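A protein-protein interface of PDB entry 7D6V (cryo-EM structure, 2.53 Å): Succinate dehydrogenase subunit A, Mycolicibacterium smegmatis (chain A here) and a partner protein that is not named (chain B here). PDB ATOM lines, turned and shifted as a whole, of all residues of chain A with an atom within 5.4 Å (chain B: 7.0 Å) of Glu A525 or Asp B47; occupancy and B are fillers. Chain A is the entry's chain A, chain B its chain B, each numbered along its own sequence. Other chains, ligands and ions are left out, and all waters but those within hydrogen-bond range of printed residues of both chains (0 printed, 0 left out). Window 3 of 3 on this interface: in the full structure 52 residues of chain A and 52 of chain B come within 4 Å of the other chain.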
ATOM      1  N   PHE A 472       4.370  25.051 -13.107  1.00  0.00           N
ATOM      2  CA  PHE A 472       3.551  25.237 -11.916  1.00  0.00           C
ATOM      3  C   PHE A 472       2.884  26.604 -11.845  1.00  0.00           C
ATOM      4  O   PHE A 472       2.059  26.822 -10.953  1.00  0.00           O
ATOM      5  CB  PHE A 472       4.386  25.015 -10.650  1.00  0.00           C
ATOM      6  CG  PHE A 472       4.573  23.570 -10.293  1.00  0.00           C
ATOM      7  CD1 PHE A 472       5.836  23.006 -10.268  1.00  0.00           C
ATOM      8  CD2 PHE A 472       3.488  22.776  -9.980  1.00  0.00           C
ATOM      9  CE1 PHE A 472       6.009  21.679  -9.937  1.00  0.00           C
ATOM     10  CE2 PHE A 472       3.657  21.450  -9.651  1.00  0.00           C
ATOM     11  CZ  PHE A 472       4.919  20.900  -9.629  1.00  0.00           C
ATOM     12  N   TYR A 482      -1.563  15.467 -20.104  1.00  0.00           N
ATOM     13  CA  TYR A 482      -2.033  14.200 -20.651  1.00  0.00           C
ATOM     14  C   TYR A 482      -2.708  14.396 -22.002  1.00  0.00           C
ATOM     15  O   TYR A 482      -2.513  13.595 -22.924  1.00  0.00           O
ATOM     16  CB  TYR A 482      -2.985  13.530 -19.661  1.00  0.00           C
ATOM     17  CG  TYR A 482      -2.333  13.137 -18.356  1.00  0.00           C
ATOM     18  CD1 TYR A 482      -1.754  11.888 -18.197  1.00  0.00           C
ATOM     19  CD2 TYR A 482      -2.294  14.014 -17.284  1.00  0.00           C
ATOM     20  CE1 TYR A 482      -1.159  11.524 -17.011  1.00  0.00           C
ATOM     21  CE2 TYR A 482      -1.697  13.657 -16.093  1.00  0.00           C
ATOM     22  CZ  TYR A 482      -1.132  12.412 -15.963  1.00  0.00           C
ATOM     23  OH  TYR A 482      -0.538  12.049 -14.780  1.00  0.00           O
ATOM     24  N   THR A 523      -0.041  23.589 -17.719  1.00  0.00           N
ATOM     25  CA  THR A 523      -0.183  23.864 -16.298  1.00  0.00           C
ATOM     26  C   THR A 523      -0.292  22.547 -15.545  1.00  0.00           C
ATOM     27  O   THR A 523      -1.029  21.649 -15.963  1.00  0.00           O
ATOM     28  CB  THR A 523      -1.408  24.736 -16.022  1.00  0.00           C
ATOM     29  OG1 THR A 523      -1.378  25.892 -16.867  1.00  0.00           O
ATOM     30  CG2 THR A 523      -1.425  25.182 -14.572  1.00  0.00           C
ATOM     31  N   VAL A 524       0.437  22.436 -14.442  1.00  0.00           N
ATOM     32  CA  VAL A 524       0.459  21.235 -13.618  1.00  0.00           C
ATOM     33  C   VAL A 524      -0.200  21.563 -12.287  1.00  0.00           C
ATOM     34  O   VAL A 524       0.130  22.573 -11.655  1.00  0.00           O
ATOM     35  CB  VAL A 524       1.892  20.716 -13.419  1.00  0.00           C
ATOM     36  CG1 VAL A 524       1.939  19.684 -12.318  1.00  0.00           C
ATOM     37  CG2 VAL A 524       2.421  20.131 -14.712  1.00  0.00           C
ATOM     38  N   GLU A 525      -1.136  20.716 -11.870  1.00  0.00           N
ATOM     39  CA  GLU A 525      -1.853  20.889 -10.615  1.00  0.00           C
ATOM     40  C   GLU A 525      -1.233  19.997  -9.548  1.00  0.00           C
ATOM     41  O   GLU A 525      -0.966  18.819  -9.796  1.00  0.00           O
ATOM     42  CB  GLU A 525      -3.336  20.556 -10.784  1.00  0.00           C
ATOM     43  CG  GLU A 525      -3.895  20.849 -12.167  1.00  0.00           C
ATOM     44  CD  GLU A 525      -3.898  22.329 -12.498  1.00  0.00           C
ATOM     45  OE1 GLU A 525      -4.023  23.148 -11.562  1.00  0.00           O
ATOM     46  OE2 GLU A 525      -3.780  22.673 -13.692  1.00  0.00           O
ATOM     47  N   GLY A 526      -1.003  20.563  -8.367  1.00  0.00           N
ATOM     48  CA  GLY A 526      -0.452  19.798  -7.267  1.00  0.00           C
ATOM     49  C   GLY A 526       0.882  20.324  -6.783  1.00  0.00           C
ATOM     50  O   GLY A 526       1.215  21.491  -7.003  1.00  0.00           O
ATOM     51  N   GLY A 527       1.656  19.472  -6.118  1.00  0.00           N
ATOM     52  CA  GLY A 527       2.952  19.878  -5.614  1.00  0.00           C
ATOM     53  C   GLY A 527       4.100  19.168  -6.296  1.00  0.00           C
ATOM     54  O   GLY A 527       3.984  18.754  -7.451  1.00  0.00           O
ATOM     55  N   PHE A 530       6.412  13.509  -5.835  1.00  0.00           N
ATOM     56  CA  PHE A 530       6.184  12.421  -6.790  1.00  0.00           C
ATOM     57  C   PHE A 530       4.915  12.685  -7.604  1.00  0.00           C
ATOM     58  O   PHE A 530       3.912  11.982  -7.506  1.00  0.00           O
ATOM     59  CB  PHE A 530       6.134  11.065  -6.079  1.00  0.00           C
ATOM     60  CG  PHE A 530       5.994   9.894  -7.014  1.00  0.00           C
ATOM     61  CD1 PHE A 530       7.096   9.465  -7.730  1.00  0.00           C
ATOM     62  CD2 PHE A 530       4.798   9.251  -7.213  1.00  0.00           C
ATOM     63  CE1 PHE A 530       7.010   8.403  -8.593  1.00  0.00           C
ATOM     64  CE2 PHE A 530       4.705   8.196  -8.094  1.00  0.00           C
ATOM     65  CZ  PHE A 530       5.814   7.771  -8.780  1.00  0.00           C
ATOM     66  N   ASN A 531       4.962  13.771  -8.377  1.00  0.00           N
ATOM     67  CA  ASN A 531       3.827  14.254  -9.150  1.00  0.00           C
ATOM     68  C   ASN A 531       3.975  13.815 -10.602  1.00  0.00           C
ATOM     69  O   ASN A 531       4.707  14.461 -11.368  1.00  0.00           O
ATOM     70  CB  ASN A 531       3.738  15.778  -9.053  1.00  0.00           C
ATOM     71  CG  ASN A 531       2.433  16.324  -9.581  1.00  0.00           C
ATOM     72  OD1 ASN A 531       1.679  15.626 -10.247  1.00  0.00           O
ATOM     73  ND2 ASN A 531       2.169  17.590  -9.296  1.00  0.00           N
ATOM     74  N   PRO A 532       3.313  12.738 -11.035  1.00  0.00           N
ATOM     75  CA  PRO A 532       3.525  12.249 -12.407  1.00  0.00           C
ATOM     76  C   PRO A 532       3.020  13.186 -13.492  1.00  0.00           C
ATOM     77  O   PRO A 532       3.503  13.092 -14.626  1.00  0.00           O
ATOM     78  CB  PRO A 532       2.769  10.915 -12.430  1.00  0.00           C
ATOM     79  CG  PRO A 532       1.829  10.982 -11.296  1.00  0.00           C
ATOM     80  CD  PRO A 532       2.425  11.860 -10.259  1.00  0.00           C
ATOM     81  N   GLY A 533       2.076  14.080 -13.197  1.00  0.00           N
ATOM     82  CA  GLY A 533       1.694  15.076 -14.185  1.00  0.00           C
ATOM     83  C   GLY A 533       2.815  16.059 -14.461  1.00  0.00           C
ATOM     84  O   GLY A 533       3.069  16.425 -15.611  1.00  0.00           O
ATOM     85  N   ARG B  12      -5.404   7.601  -0.684  1.00  0.00           N
ATOM     86  CA  ARG B  12      -4.655   8.828  -0.928  1.00  0.00           C
ATOM     87  C   ARG B  12      -4.027   9.323   0.367  1.00  0.00           C
ATOM     88  O   ARG B  12      -4.643   9.247   1.431  1.00  0.00           O
ATOM     89  CB  ARG B  12      -5.549   9.935  -1.507  1.00  0.00           C
ATOM     90  CG  ARG B  12      -6.400   9.533  -2.690  1.00  0.00           C
ATOM     91  CD  ARG B  12      -5.575   9.241  -3.925  1.00  0.00           C
ATOM     92  NE  ARG B  12      -4.567  10.261  -4.190  1.00  0.00           N
ATOM     93  CZ  ARG B  12      -4.751  11.317  -4.975  1.00  0.00           C
ATOM     94  NH1 ARG B  12      -3.772  12.187  -5.159  1.00  0.00           N
ATOM     95  NH2 ARG B  12      -5.918  11.509  -5.569  1.00  0.00           N
ATOM     96  N   GLN B  41      -5.902   8.827 -13.732  1.00  0.00           N
ATOM     97  CA  GLN B  41      -4.864   9.853 -13.760  1.00  0.00           C
ATOM     98  C   GLN B  41      -5.105  10.860 -14.873  1.00  0.00           C
ATOM     99  O   GLN B  41      -4.974  12.071 -14.666  1.00  0.00           O
ATOM    100  CB  GLN B  41      -3.496   9.204 -13.936  1.00  0.00           C
ATOM    101  CG  GLN B  41      -2.680   9.107 -12.675  1.00  0.00           C
ATOM    102  CD  GLN B  41      -1.298   8.567 -12.938  1.00  0.00           C
ATOM    103  OE1 GLN B  41      -1.032   8.012 -14.000  1.00  0.00           O
ATOM    104  NE2 GLN B  41      -0.406   8.732 -11.974  1.00  0.00           N
ATOM    105  N   GLN B  44      -9.128  12.464 -13.874  1.00  0.00           N
ATOM    106  CA  GLN B  44      -9.567  13.033 -12.604  1.00  0.00           C
ATOM    107  C   GLN B  44      -8.435  13.413 -11.665  1.00  0.00           C
ATOM    108  O   GLN B  44      -8.504  14.466 -11.027  1.00  0.00           O
ATOM    109  CB  GLN B  44     -10.503  12.050 -11.888  1.00  0.00           C
ATOM    110  CG  GLN B  44     -11.849  11.872 -12.564  1.00  0.00           C
ATOM    111  CD  GLN B  44     -12.684  10.780 -11.930  1.00  0.00           C
ATOM    112  OE1 GLN B  44     -12.920   9.736 -12.532  1.00  0.00           O
ATOM    113  NE2 GLN B  44     -13.140  11.018 -10.709  1.00  0.00           N
ATOM    114  N   THR B  45      -7.389  12.591 -11.558  1.00  0.00           N
ATOM    115  CA  THR B  45      -6.338  12.754 -10.555  1.00  0.00           C
ATOM    116  C   THR B  45      -4.981  12.791 -11.245  1.00  0.00           C
ATOM    117  O   THR B  45      -4.257  11.785 -11.266  1.00  0.00           O
ATOM    118  CB  THR B  45      -6.378  11.633  -9.518  1.00  0.00           C
ATOM    119  OG1 THR B  45      -6.023  10.393 -10.139  1.00  0.00           O
ATOM    120  CG2 THR B  45      -7.764  11.510  -8.918  1.00  0.00           C
ATOM    121  N   PRO B  46      -4.597  13.937 -11.811  1.00  0.00           N
ATOM    122  CA  PRO B  46      -3.311  14.010 -12.524  1.00  0.00           C
ATOM    123  C   PRO B  46      -2.102  13.740 -11.645  1.00  0.00           C
ATOM    124  O   PRO B  46      -1.083  13.246 -12.141  1.00  0.00           O
ATOM    125  CB  PRO B  46      -3.294  15.444 -13.073  1.00  0.00           C
ATOM    126  CG  PRO B  46      -4.684  15.956 -12.919  1.00  0.00           C
ATOM    127  CD  PRO B  46      -5.280  15.237 -11.768  1.00  0.00           C
ATOM    128  N   ASP B  47      -2.182  14.050 -10.350  1.00  0.00           N
ATOM    129  CA  ASP B  47      -1.051  13.949  -9.437  1.00  0.00           C
ATOM    130  C   ASP B  47      -1.085  12.681  -8.589  1.00  0.00           C
ATOM    131  O   ASP B  47      -0.450  12.633  -7.533  1.00  0.00           O
ATOM    132  CB  ASP B  47      -0.998  15.177  -8.531  1.00  0.00           C
ATOM    133  CG  ASP B  47      -2.312  15.438  -7.834  1.00  0.00           C
ATOM    134  OD1 ASP B  47      -3.346  14.927  -8.310  1.00  0.00           O
ATOM    135  OD2 ASP B  47      -2.312  16.134  -6.801  1.00  0.00           O
ATOM    136  N   LEU B  48      -1.813  11.656  -9.022  1.00  0.00           N
ATOM    137  CA  LEU B  48      -1.902  10.411  -8.271  1.00  0.00           C
ATOM    138  C   LEU B  48      -0.633   9.584  -8.448  1.00  0.00           C
ATOM    139  O   LEU B  48      -0.184   9.354  -9.572  1.00  0.00           O
ATOM    140  CB  LEU B  48      -3.122   9.609  -8.718  1.00  0.00           C
ATOM    141  CG  LEU B  48      -3.215   8.161  -8.247  1.00  0.00           C
ATOM    142  CD1 LEU B  48      -3.676   8.115  -6.813  1.00  0.00           C
ATOM    143  CD2 LEU B  48      -4.165   7.391  -9.137  1.00  0.00           C
ATOM    144  N   ALA B  49      -0.078   9.114  -7.332  1.00  0.00           N
ATOM    145  CA  ALA B  49       1.208   8.424  -7.322  1.00  0.00           C
ATOM    146  C   ALA B  49       1.037   6.939  -7.629  1.00  0.00           C
ATOM    147  O   ALA B  49       0.257   6.254  -6.964  1.00  0.00           O
ATOM    148  CB  ALA B  49       1.863   8.612  -5.955  1.00  0.00           C
ATOM    149  N   VAL B  50       1.765   6.432  -8.633  1.00  0.00           N
ATOM    150  CA  VAL B  50       1.532   5.067  -9.113  1.00  0.00           C
ATOM    151  C   VAL B  50       2.798   4.214  -9.162  1.00  0.00           C
ATOM    152  O   VAL B  50       2.844   3.140  -8.553  1.00  0.00           O
ATOM    153  CB  VAL B  50       0.852   5.082 -10.493  1.00  0.00           C
ATOM    154  CG1 VAL B  50       0.594   3.666 -10.966  1.00  0.00           C
ATOM    155  CG2 VAL B  50      -0.444   5.844 -10.426  1.00  0.00           C
ATOM    156  N   ARG B  99       3.908   8.102  -1.109  1.00  0.00           N
ATOM    157  CA  ARG B  99       2.682   8.825  -1.394  1.00  0.00           C
ATOM    158  C   ARG B  99       1.623   7.786  -1.749  1.00  0.00           C
ATOM    159  O   ARG B  99       1.751   6.616  -1.376  1.00  0.00           O
ATOM    160  CB  ARG B  99       2.921   9.886  -2.479  1.00  0.00           C
ATOM    161  CG  ARG B  99       2.046  11.108  -2.311  1.00  0.00           C
ATOM    162  CD  ARG B  99       2.030  11.963  -3.548  1.00  0.00           C
ATOM    163  NE  ARG B  99       0.935  12.922  -3.511  1.00  0.00           N
ATOM    164  CZ  ARG B  99       0.415  13.497  -4.585  1.00  0.00           C
ATOM    165  NH1 ARG B  99       0.895  13.214  -5.786  1.00  0.00           N
ATOM    166  NH2 ARG B  99      -0.585  14.356  -4.457  1.00  0.00           N
ATOM    167  N   ASP B 100       0.597   8.203  -2.493  1.00  0.00           N
ATOM    168  CA  ASP B 100      -0.664   7.472  -2.592  1.00  0.00           C
ATOM    169  C   ASP B 100      -0.505   5.961  -2.749  1.00  0.00           C
ATOM    170  O   ASP B 100      -0.933   5.193  -1.885  1.00  0.00           O
ATOM    171  CB  ASP B 100      -1.474   8.044  -3.758  1.00  0.00           C
ATOM    172  CG  ASP B 100      -1.462   9.554  -3.785  1.00  0.00           C
ATOM    173  OD1 ASP B 100      -1.835  10.172  -2.769  1.00  0.00           O
ATOM    174  OD2 ASP B 100      -1.073  10.129  -4.819  1.00  0.00           O
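N of Gly A533 sits at hydrogen-bond distance from O of Pro B46 (3.4 Å).
The side-chain hydroxyl of Tyr A482 sits at hydrogen-bond distance from the backbone carbonyl oxygen of Pro B46, 2.9 Å away.
Among the printed residues, pairs that only touch across the chains: Tyr A482 with Gln B41 (3.9 Å), Glu A525 with Asp B47 (3.9 Å), Phe A530 with Ala B49 (3.3 Å), Phe A530 with Val B50 (3.5 Å), Phe A530 with Arg B99 (3.7 Å), Asn A531 with Asp B47 (3.2 Å), Pro A532 with Gln B41 (3.2 Å), Pro A532 with Pro B46 (3.8 Å), Pro A532 with Asp B47 (3.97 Å) and Pro A532 with Leu B48 (3.1 Å).
Of the printed residues of chain B, Tyr A482 touches Gln B41 (3.9 Å) and Pro B46 (2.9 Å).
Glu A525 touches one residue of chain B.
Of the printed residues of chain B, Asn A531 touches Asp B47 (3.2 Å).
Printed residues of chain A within 4 Å of Gln B41: Tyr A482 and Pro A532.
Printed residues of chain A within 4 Å of Pro B46: Tyr A482, Pro A532 and Gly A533.
Asp B47 touches just these residues of chain A: Glu A525, Asn A531 and Pro A532.
Printed residues of chain A within 4 Å of Arg B99: Phe A530.
The nearest residue of chain B that does not touch Glu A525 is Pro B46 (5.0 Å).
The nearest residue of chain A that does not touch Asp B47 is Gly A526 (4.1 Å).
Printed residues of chain B that touch a printed residue of chain A: Gln B41, Pro B46, Asp B47, Leu B48, Ala B49, Val B50 and Arg B99.
Printed residues of chain A that touch a printed residue of chain B: Tyr A482, Glu A525, Phe A530, Asn A531, Pro A532 and Gly A533.
The backbone carbonyl oxygen (O) of Leu B48 lies within hydrogen-bond range of the side-chain amide nitrogen (NE2) of Gln B41 (2.5 Å).
The guanidinium group (NH2) of Arg B99 lies within salt-bridge range of the side-chain carboxylate (OD2) of Asp B47 (3.4 Å).
The side-chain amide nitrogen (ND2) of Asn A531 is in hydrogen-bond range of the backbone carbonyl oxygen (O) of Glu A525 (3.4 Å).
The side-chain amide oxygen (OD1) of Asn A531 sits close to the backbone NH (N) of Gly A533, 3.4 Å away.
The guanidinium group (NE) of Arg B99 is in salt-bridge range of the side-chain carboxylate (OD2) of Asp B100 (3.7 Å).
OD2 of Asp B100 is in hydrogen-bond range of N of Ala B49 (2.9 Å).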
